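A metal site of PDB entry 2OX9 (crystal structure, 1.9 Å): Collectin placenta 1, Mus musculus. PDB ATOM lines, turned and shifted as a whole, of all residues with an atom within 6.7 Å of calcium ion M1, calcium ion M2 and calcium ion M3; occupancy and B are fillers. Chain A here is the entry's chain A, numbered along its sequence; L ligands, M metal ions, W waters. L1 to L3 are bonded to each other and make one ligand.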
ATOM      1  N   ASP A  68     -13.084 -29.873 -20.831  1.00  0.00           N
ATOM      2  CA  ASP A  68     -11.680 -29.492 -20.939  1.00  0.00           C
ATOM      3  C   ASP A  68     -10.961 -30.013 -19.691  1.00  0.00           C
ATOM      4  O   ASP A  68     -10.059 -29.366 -19.157  1.00  0.00           O
ATOM      5  CB  ASP A  68     -11.528 -27.959 -21.098  1.00  0.00           C
ATOM      6  CG  ASP A  68     -11.796 -27.204 -19.806  1.00  0.00           C
ATOM      7  OD1 ASP A  68     -12.526 -27.708 -18.949  1.00  0.00           O
ATOM      8  OD2 ASP A  68     -11.265 -26.076 -19.663  1.00  0.00           O
ATOM      9  N   SER A  69     -11.386 -31.191 -19.248  1.00  0.00           N
ATOM     10  CA  SER A  69     -10.810 -31.857 -18.079  1.00  0.00           C
ATOM     11  C   SER A  69      -9.425 -32.416 -18.379  1.00  0.00           C
ATOM     12  O   SER A  69      -8.557 -32.408 -17.513  1.00  0.00           O
ATOM     13  CB  SER A  69     -11.707 -33.004 -17.617  1.00  0.00           C
ATOM     14  OG  SER A  69     -12.974 -32.542 -17.183  1.00  0.00           O
ATOM     15  N   GLN A  71      -7.150 -31.234 -20.436  1.00  0.00           N
ATOM     16  CA  GLN A  71      -6.197 -30.135 -20.404  1.00  0.00           C
ATOM     17  C   GLN A  71      -6.986 -28.825 -20.397  1.00  0.00           C
ATOM     18  O   GLN A  71      -7.650 -28.480 -21.371  1.00  0.00           O
ATOM     19  CB  GLN A  71      -5.294 -30.188 -21.633  1.00  0.00           C
ATOM     20  CG  GLN A  71      -4.078 -29.272 -21.552  1.00  0.00           C
ATOM     21  CD  GLN A  71      -3.131 -29.443 -22.728  1.00  0.00           C
ATOM     22  OE1 GLN A  71      -2.665 -30.545 -23.013  1.00  0.00           O
ATOM     23  NE2 GLN A  71      -2.837 -28.343 -23.414  1.00  0.00           N
ATOM     24  N   GLU A  72      -6.921 -28.113 -19.279  1.00  0.00           N
ATOM     25  CA  GLU A  72      -7.627 -26.848 -19.126  1.00  0.00           C
ATOM     26  C   GLU A  72      -7.553 -25.981 -20.391  1.00  0.00           C
ATOM     27  O   GLU A  72      -6.479 -25.809 -20.974  1.00  0.00           O
ATOM     28  CB  GLU A  72      -7.074 -26.089 -17.920  1.00  0.00           C
ATOM     29  CG  GLU A  72      -7.799 -24.802 -17.555  1.00  0.00           C
ATOM     30  CD  GLU A  72      -9.281 -25.016 -17.285  1.00  0.00           C
ATOM     31  OE1 GLU A  72      -9.623 -26.050 -16.677  1.00  0.00           O
ATOM     32  OE2 GLU A  72     -10.091 -24.157 -17.663  1.00  0.00           O
ATOM     33  N   SER A  73      -8.703 -25.455 -20.800  1.00  0.00           N
ATOM     34  CA  SER A  73      -8.841 -24.596 -21.976  1.00  0.00           C
ATOM     35  C   SER A  73      -8.819 -25.293 -23.321  1.00  0.00           C
ATOM     36  O   SER A  73      -9.014 -24.664 -24.356  1.00  0.00           O
ATOM     37  CB  SER A  73      -7.793 -23.477 -21.963  1.00  0.00           C
ATOM     38  OG  SER A  73      -8.103 -22.521 -20.964  1.00  0.00           O
ATOM     39  N   TRP A  75     -10.880 -27.547 -25.132  1.00  0.00           N
ATOM     40  CA  TRP A  75     -12.205 -28.141 -25.205  1.00  0.00           C
ATOM     41  C   TRP A  75     -12.390 -29.145 -26.336  1.00  0.00           C
ATOM     42  O   TRP A  75     -12.070 -28.851 -27.480  1.00  0.00           O
ATOM     43  CB  TRP A  75     -13.270 -27.040 -25.298  1.00  0.00           C
ATOM     44  CG  TRP A  75     -13.385 -26.225 -24.048  1.00  0.00           C
ATOM     45  CD1 TRP A  75     -12.644 -25.123 -23.720  1.00  0.00           C
ATOM     46  CD2 TRP A  75     -14.251 -26.473 -22.939  1.00  0.00           C
ATOM     47  NE1 TRP A  75     -13.011 -24.675 -22.474  1.00  0.00           N
ATOM     48  CE2 TRP A  75     -13.994 -25.486 -21.972  1.00  0.00           C
ATOM     49  CE3 TRP A  75     -15.228 -27.452 -22.670  1.00  0.00           C
ATOM     50  CZ2 TRP A  75     -14.676 -25.428 -20.753  1.00  0.00           C
ATOM     51  CZ3 TRP A  75     -15.905 -27.391 -21.459  1.00  0.00           C
ATOM     52  CH2 TRP A  75     -15.621 -26.394 -20.508  1.00  0.00           C
ATOM     53  N   GLY A  91     -17.534 -13.870 -22.609  1.00  0.00           N
ATOM     54  CA  GLY A  91     -16.945 -13.908 -21.285  1.00  0.00           C
ATOM     55  C   GLY A  91     -16.693 -15.334 -20.825  1.00  0.00           C
ATOM     56  O   GLY A  91     -15.884 -15.579 -19.929  1.00  0.00           O
ATOM     57  N   GLN A  92     -17.405 -16.280 -21.444  1.00  0.00           N
ATOM     58  CA  GLN A  92     -17.254 -17.691 -21.117  1.00  0.00           C
ATOM     59  C   GLN A  92     -16.374 -18.347 -22.180  1.00  0.00           C
ATOM     60  O   GLN A  92     -16.324 -17.891 -23.311  1.00  0.00           O
ATOM     61  CB  GLN A  92     -18.620 -18.378 -21.092  1.00  0.00           C
ATOM     62  CG  GLN A  92     -19.542 -17.836 -20.041  1.00  0.00           C
ATOM     63  CD  GLN A  92     -18.864 -17.766 -18.689  1.00  0.00           C
ATOM     64  OE1 GLN A  92     -18.406 -18.773 -18.156  1.00  0.00           O
ATOM     65  NE2 GLN A  92     -18.791 -16.558 -18.133  1.00  0.00           N
ATOM     66  N   PRO A  93     -15.659 -19.431 -21.821  1.00  0.00           N
ATOM     67  CA  PRO A  93     -15.598 -20.098 -20.511  1.00  0.00           C
ATOM     68  C   PRO A  93     -14.719 -19.317 -19.542  1.00  0.00           C
ATOM     69  O   PRO A  93     -13.689 -18.779 -19.931  1.00  0.00           O
ATOM     70  CB  PRO A  93     -15.028 -21.477 -20.849  1.00  0.00           C
ATOM     71  CG  PRO A  93     -14.152 -21.193 -22.038  1.00  0.00           C
ATOM     72  CD  PRO A  93     -14.974 -20.247 -22.851  1.00  0.00           C
ATOM     73  N   ASP A  94     -15.128 -19.235 -18.279  1.00  0.00           N
ATOM     74  CA  ASP A  94     -14.351 -18.469 -17.306  1.00  0.00           C
ATOM     75  C   ASP A  94     -13.637 -19.304 -16.248  1.00  0.00           C
ATOM     76  O   ASP A  94     -12.890 -18.757 -15.439  1.00  0.00           O
ATOM     77  CB  ASP A  94     -15.244 -17.420 -16.647  1.00  0.00           C
ATOM     78  CG  ASP A  94     -16.406 -18.030 -15.881  1.00  0.00           C
ATOM     79  OD1 ASP A  94     -16.592 -19.258 -15.964  1.00  0.00           O
ATOM     80  OD2 ASP A  94     -17.129 -17.276 -15.192  1.00  0.00           O
ATOM     81  N   ASN A  95     -13.877 -20.612 -16.248  1.00  0.00           N
ATOM     82  CA  ASN A  95     -13.258 -21.533 -15.287  1.00  0.00           C
ATOM     83  C   ASN A  95     -13.382 -20.992 -13.859  1.00  0.00           C
ATOM     84  O   ASN A  95     -12.433 -21.033 -13.078  1.00  0.00           O
ATOM     85  CB  ASN A  95     -11.774 -21.722 -15.655  1.00  0.00           C
ATOM     86  CG  ASN A  95     -11.231 -23.076 -15.219  1.00  0.00           C
ATOM     87  OD1 ASN A  95     -11.860 -24.120 -15.451  1.00  0.00           O
ATOM     88  ND2 ASN A  95     -10.057 -23.068 -14.601  1.00  0.00           N
ATOM     89  N   TRP A  96     -14.562 -20.506 -13.524  1.00  0.00           N
ATOM     90  CA  TRP A  96     -14.846 -19.934 -12.209  1.00  0.00           C
ATOM     91  C   TRP A  96     -14.435 -20.869 -11.071  1.00  0.00           C
ATOM     92  O   TRP A  96     -14.712 -22.065 -11.109  1.00  0.00           O
ATOM     93  CB  TRP A  96     -16.336 -19.617 -12.105  1.00  0.00           C
ATOM     94  CG  TRP A  96     -16.694 -18.580 -11.101  1.00  0.00           C
ATOM     95  CD1 TRP A  96     -17.424 -18.757  -9.963  1.00  0.00           C
ATOM     96  CD2 TRP A  96     -16.377 -17.178 -11.162  1.00  0.00           C
ATOM     97  NE1 TRP A  96     -17.582 -17.547  -9.312  1.00  0.00           N
ATOM     98  CE2 TRP A  96     -16.949 -16.571 -10.026  1.00  0.00           C
ATOM     99  CE3 TRP A  96     -15.659 -16.381 -12.064  1.00  0.00           C
ATOM    100  CZ2 TRP A  96     -16.838 -15.199  -9.777  1.00  0.00           C
ATOM    101  CZ3 TRP A  96     -15.541 -15.017 -11.814  1.00  0.00           C
ATOM    102  CH2 TRP A  96     -16.136 -14.446 -10.670  1.00  0.00           C
ATOM    103  N   SER A  98     -11.304 -21.667 -10.122  1.00  0.00           N
ATOM    104  CA  SER A  98     -10.067 -22.416 -10.346  1.00  0.00           C
ATOM    105  C   SER A  98      -9.071 -22.227  -9.208  1.00  0.00           C
ATOM    106  O   SER A  98      -8.185 -23.058  -9.009  1.00  0.00           O
ATOM    107  CB  SER A  98      -9.413 -21.978 -11.658  1.00  0.00           C
ATOM    108  OG  SER A  98      -9.121 -20.588 -11.652  1.00  0.00           O
ATOM    109  N   GLY A 101      -9.967 -25.127  -6.711  1.00  0.00           N
ATOM    110  CA  GLY A 101     -10.265 -26.454  -7.235  1.00  0.00           C
ATOM    111  C   GLY A 101      -9.971 -26.566  -8.722  1.00  0.00           C
ATOM    112  O   GLY A 101      -9.212 -25.758  -9.265  1.00  0.00           O
ATOM    113  N   PRO A 102     -10.570 -27.543  -9.422  1.00  0.00           N
ATOM    114  CA  PRO A 102     -10.355 -27.737 -10.856  1.00  0.00           C
ATOM    115  C   PRO A 102     -11.087 -26.747 -11.758  1.00  0.00           C
ATOM    116  O   PRO A 102     -10.921 -26.764 -12.983  1.00  0.00           O
ATOM    117  CB  PRO A 102     -10.828 -29.178 -11.074  1.00  0.00           C
ATOM    118  CG  PRO A 102     -11.957 -29.273 -10.102  1.00  0.00           C
ATOM    119  CD  PRO A 102     -11.411 -28.612  -8.854  1.00  0.00           C
ATOM    120  N   GLY A 103     -11.911 -25.893 -11.139  1.00  0.00           N
ATOM    121  CA  GLY A 103     -12.648 -24.909 -11.896  1.00  0.00           C
ATOM    122  C   GLY A 103     -13.903 -25.461 -12.548  1.00  0.00           C
ATOM    123  O   GLY A 103     -14.642 -26.236 -11.940  1.00  0.00           O
ATOM    124  N   GLU A 104     -14.135 -25.067 -13.795  1.00  0.00           N
ATOM    125  CA  GLU A 104     -15.304 -25.514 -14.563  1.00  0.00           C
ATOM    126  C   GLU A 104     -14.784 -26.194 -15.814  1.00  0.00           C
ATOM    127  O   GLU A 104     -14.198 -25.554 -16.690  1.00  0.00           O
ATOM    128  CB  GLU A 104     -16.185 -24.309 -14.924  1.00  0.00           C
ATOM    129  CG  GLU A 104     -16.657 -23.526 -13.686  1.00  0.00           C
ATOM    130  CD  GLU A 104     -17.659 -22.435 -14.009  1.00  0.00           C
ATOM    131  OE1 GLU A 104     -17.303 -21.480 -14.731  1.00  0.00           O
ATOM    132  OE2 GLU A 104     -18.814 -22.526 -13.543  1.00  0.00           O
ATOM    133  N   ASP A 105     -15.023 -27.496 -15.925  1.00  0.00           N
ATOM    134  CA  ASP A 105     -14.523 -28.244 -17.054  1.00  0.00           C
ATOM    135  C   ASP A 105     -15.593 -28.998 -17.854  1.00  0.00           C
ATOM    136  O   ASP A 105     -15.266 -29.871 -18.668  1.00  0.00           O
ATOM    137  CB  ASP A 105     -13.465 -29.247 -16.569  1.00  0.00           C
ATOM    138  CG  ASP A 105     -12.324 -28.575 -15.811  1.00  0.00           C
ATOM    139  OD1 ASP A 105     -12.257 -27.322 -15.804  1.00  0.00           O
ATOM    140  OD2 ASP A 105     -11.503 -29.308 -15.220  1.00  0.00           O
ATOM    141  N   CYS A 106     -16.852 -28.666 -17.610  1.00  0.00           N
ATOM    142  CA  CYS A 106     -17.969 -29.312 -18.280  1.00  0.00           C
ATOM    143  C   CYS A 106     -18.862 -28.247 -18.922  1.00  0.00           C
ATOM    144  O   CYS A 106     -19.152 -27.244 -18.293  1.00  0.00           O
ATOM    145  CB  CYS A 106     -18.732 -30.172 -17.257  1.00  0.00           C
ATOM    146  SG  CYS A 106     -17.822 -31.704 -16.831  1.00  0.00           S
ATOM    147  N   ASN A 116     -21.928 -22.328 -21.578  1.00  0.00           N
ATOM    148  CA  ASN A 116     -21.271 -21.893 -20.371  1.00  0.00           C
ATOM    149  C   ASN A 116     -20.559 -23.088 -19.759  1.00  0.00           C
ATOM    150  O   ASN A 116     -21.007 -24.219 -19.903  1.00  0.00           O
ATOM    151  CB  ASN A 116     -22.278 -21.347 -19.371  1.00  0.00           C
ATOM    152  CG  ASN A 116     -21.672 -21.147 -18.009  1.00  0.00           C
ATOM    153  OD1 ASN A 116     -20.636 -20.486 -17.875  1.00  0.00           O
ATOM    154  ND2 ASN A 116     -22.306 -21.708 -16.990  1.00  0.00           N
ATOM    155  N   ASP A 117     -19.443 -22.842 -19.088  1.00  0.00           N
ATOM    156  CA  ASP A 117     -18.718 -23.917 -18.442  1.00  0.00           C
ATOM    157  C   ASP A 117     -19.168 -23.982 -16.990  1.00  0.00           C
ATOM    158  O   ASP A 117     -19.292 -22.947 -16.319  1.00  0.00           O
ATOM    159  CB  ASP A 117     -17.187 -23.681 -18.557  1.00  0.00           C
ATOM    160  CG  ASP A 117     -16.749 -22.317 -18.042  1.00  0.00           C
ATOM    161  OD1 ASP A 117     -17.549 -21.355 -18.080  1.00  0.00           O
ATOM    162  OD2 ASP A 117     -15.577 -22.190 -17.614  1.00  0.00           O
ATOM    163  N   PHE A 118     -19.470 -25.189 -16.521  1.00  0.00           N
ATOM    164  CA  PHE A 118     -19.923 -25.401 -15.148  1.00  0.00           C
ATOM    165  C   PHE A 118     -18.958 -26.355 -14.449  1.00  0.00           C
ATOM    166  O   PHE A 118     -18.167 -27.046 -15.093  1.00  0.00           O
ATOM    167  CB  PHE A 118     -21.291 -26.096 -15.078  1.00  0.00           C
ATOM    168  CG  PHE A 118     -22.402 -25.376 -15.793  1.00  0.00           C
ATOM    169  CD1 PHE A 118     -22.570 -25.526 -17.161  1.00  0.00           C
ATOM    170  CD2 PHE A 118     -23.342 -24.647 -15.076  1.00  0.00           C
ATOM    171  CE1 PHE A 118     -23.655 -24.953 -17.811  1.00  0.00           C
ATOM    172  CE2 PHE A 118     -24.439 -24.071 -15.719  1.00  0.00           C
ATOM    173  CZ  PHE A 118     -24.595 -24.225 -17.094  1.00  0.00           C
HETATM  174  C1  LIG L   1     -24.230 -14.739 -15.435  1.00  0.00           C
HETATM  175  C2  LIG L   1     -23.305 -13.552 -15.761  1.00  0.00           C
HETATM  176  C3  LIG L   1     -21.853 -14.023 -15.805  1.00  0.00           C
HETATM  177  C4  LIG L   1     -21.709 -15.183 -16.783  1.00  0.00           C
HETATM  178  C5  LIG L   1     -22.664 -16.315 -16.389  1.00  0.00           C
HETATM  179  C6  LIG L   1     -22.619 -17.477 -17.381  1.00  0.00           C
HETATM  180  O1  LIG L   1     -23.448 -12.546 -14.773  1.00  0.00           O
HETATM  181  O2  LIG L   1     -21.012 -12.947 -16.193  1.00  0.00           O
HETATM  182  O3  LIG L   1     -22.004 -14.737 -18.098  1.00  0.00           O
HETATM  183  O4  LIG L   1     -24.025 -15.824 -16.343  1.00  0.00           O
HETATM  184  C1  LG2 L   2     -27.032 -15.978 -11.935  1.00  0.00           C
HETATM  185  C2  LG2 L   2     -25.966 -15.099 -12.581  1.00  0.00           C
HETATM  186  C3  LG2 L   2     -25.126 -15.920 -13.553  1.00  0.00           C
HETATM  187  C4  LG2 L   2     -24.535 -17.127 -12.822  1.00  0.00           C
HETATM  188  C5  LG2 L   2     -25.654 -17.928 -12.163  1.00  0.00           C
HETATM  189  C6  LG2 L   2     -25.115 -19.081 -11.327  1.00  0.00           C
HETATM  190  C7  LG2 L   2     -26.112 -12.758 -13.133  1.00  0.00           C
HETATM  191  C8  LG2 L   2     -27.036 -11.611 -13.496  1.00  0.00           C
HETATM  192  N1  LG2 L   2     -26.604 -13.988 -13.270  1.00  0.00           N
HETATM  193  O1  LG2 L   2     -27.732 -15.238 -10.998  1.00  0.00           O
HETATM  194  O2  LG2 L   2     -24.068 -15.114 -14.098  1.00  0.00           O
HETATM  195  O3  LG2 L   2     -23.815 -17.959 -13.748  1.00  0.00           O
HETATM  196  O4  LG2 L   2     -26.408 -17.078 -11.262  1.00  0.00           O
HETATM  197  O5  LG2 L   2     -24.185 -18.621 -10.366  1.00  0.00           O
HETATM  198  O6  LG2 L   2     -24.958 -12.529 -12.746  1.00  0.00           O
HETATM  199  C1  LG3 L   3     -22.554 -18.376 -13.348  1.00  0.00           C
HETATM  200  C2  LG3 L   3     -22.117 -19.552 -14.224  1.00  0.00           C
HETATM  201  C3  LG3 L   3     -20.678 -19.960 -13.883  1.00  0.00           C
HETATM  202  C4  LG3 L   3     -19.745 -18.752 -13.917  1.00  0.00           C
HETATM  203  C5  LG3 L   3     -20.307 -17.606 -13.070  1.00  0.00           C
HETATM  204  C6  LG3 L   3     -19.480 -16.333 -13.181  1.00  0.00           C
HETATM  205  O1  LG3 L   3     -22.984 -20.646 -14.011  1.00  0.00           O
HETATM  206  O2  LG3 L   3     -20.247 -20.926 -14.824  1.00  0.00           O
HETATM  207  O3  LG3 L   3     -19.577 -18.319 -15.261  1.00  0.00           O
HETATM  208  O4  LG3 L   3     -21.649 -17.275 -13.497  1.00  0.00           O
HETATM  209  O5  LG3 L   3     -19.814 -15.411 -12.161  1.00  0.00           O
HETATM  210 CA    CA M   1     -12.022 -25.553 -17.433  1.00  0.00          CA
HETATM  211 CA    CA M   2     -18.663 -20.543 -16.491  1.00  0.00          CA
HETATM  212 CA    CA M   3      -9.956 -27.591 -14.986  1.00  0.00          CA
HETATM  213  O   HOH W   1      -8.239 -26.031 -14.021  1.00  0.00           O
HETATM  214  O   HOH W   2      -8.905 -28.623 -16.508  1.00  0.00           O
HETATM  215  O   HOH W   3     -13.098 -23.220 -18.020  1.00  0.00           O
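Water W2 is bound to calcium ion M3 (2.1 Å).
Calcium ion M3 is bound by the side-chain carboxylate (OE1) of Glu 72.
Calcium ion M3 is bound by the side-chain carboxylate (OD2) of Asp 105, 2.3 Å away.
The backbone carbonyl oxygen (O) of Pro 102 binds calcium ion M3 (2.4 Å).
OD1 of Asp 105 binds calcium ion M3, 2.5 Å away.
Calcium ion M3 is bound by water W1, 2.5 Å away.
Calcium ion M3 has six donor atoms within binding distance.
Five residues have an atom within 4 Å of calcium ion M1: Asp 68, Glu 72, Asn 95, Glu 104 and Asp 105.
N of Asn 95 sits at hydrogen-bond distance from OD2 of Asp 117 (2.7 Å).
The side-chain carboxylate (OE1) of Glu 104 lies close to the backbone NH (N) of Trp 96 (3.1 Å).
O of Phe 118 sits at hydrogen-bond distance from N of Asp 105.
OD2 of Asp 68 lies close to N of Ser 73 (2.9 Å).
The backbone NH (N) of Trp 96 sits close to the side-chain carboxylate (OD1) of Asp 94.
Water W3 lies within hydrogen-bond range of OD2 of Asp 117 (2.7 Å) and N of Asn 95 (3.2 Å).
Calcium ion M2 is bound by OD1 of Asp 117, O2 of LG3 L3, OD1 of Asn 116, OE1 of Glu 104, OE1 of Gln 92, O of Asp 117, OD1 of Asp 94 and O3 of LG3 L3.
Calcium ion M2 has eight donor atoms within binding distance.
Calcium ion M1 is bound by the backbone carbonyl oxygen (O) of Glu 104 (2.3 Å), the side-chain carboxylate (OE2) of Glu 72 (2.4 Å), the side-chain carboxylate (OD2) of Asp 68 (2.4 Å), the side-chain carboxylate (OD1) of Asp 105 (2.4 Å), the side-chain amide oxygen (OD1) of Asn 95 (2.5 Å), the side-chain carboxylate (OE1) of Glu 72 (2.6 Å), water W3 (2.6 Å) and the side-chain carboxylate (OD1) of Asp 68 (2.7 Å).
Five residues have an atom within 4 Å of calcium ion M2: Gln 92, Asp 94, Glu 104, Asn 116 and Asp 117.
The nearest printed residue that does not touch calcium ion M2 is Phe 118 (4.7 Å).
The nearest printed residue that does not touch calcium ion M3 is Asp 68 (4.5 Å).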
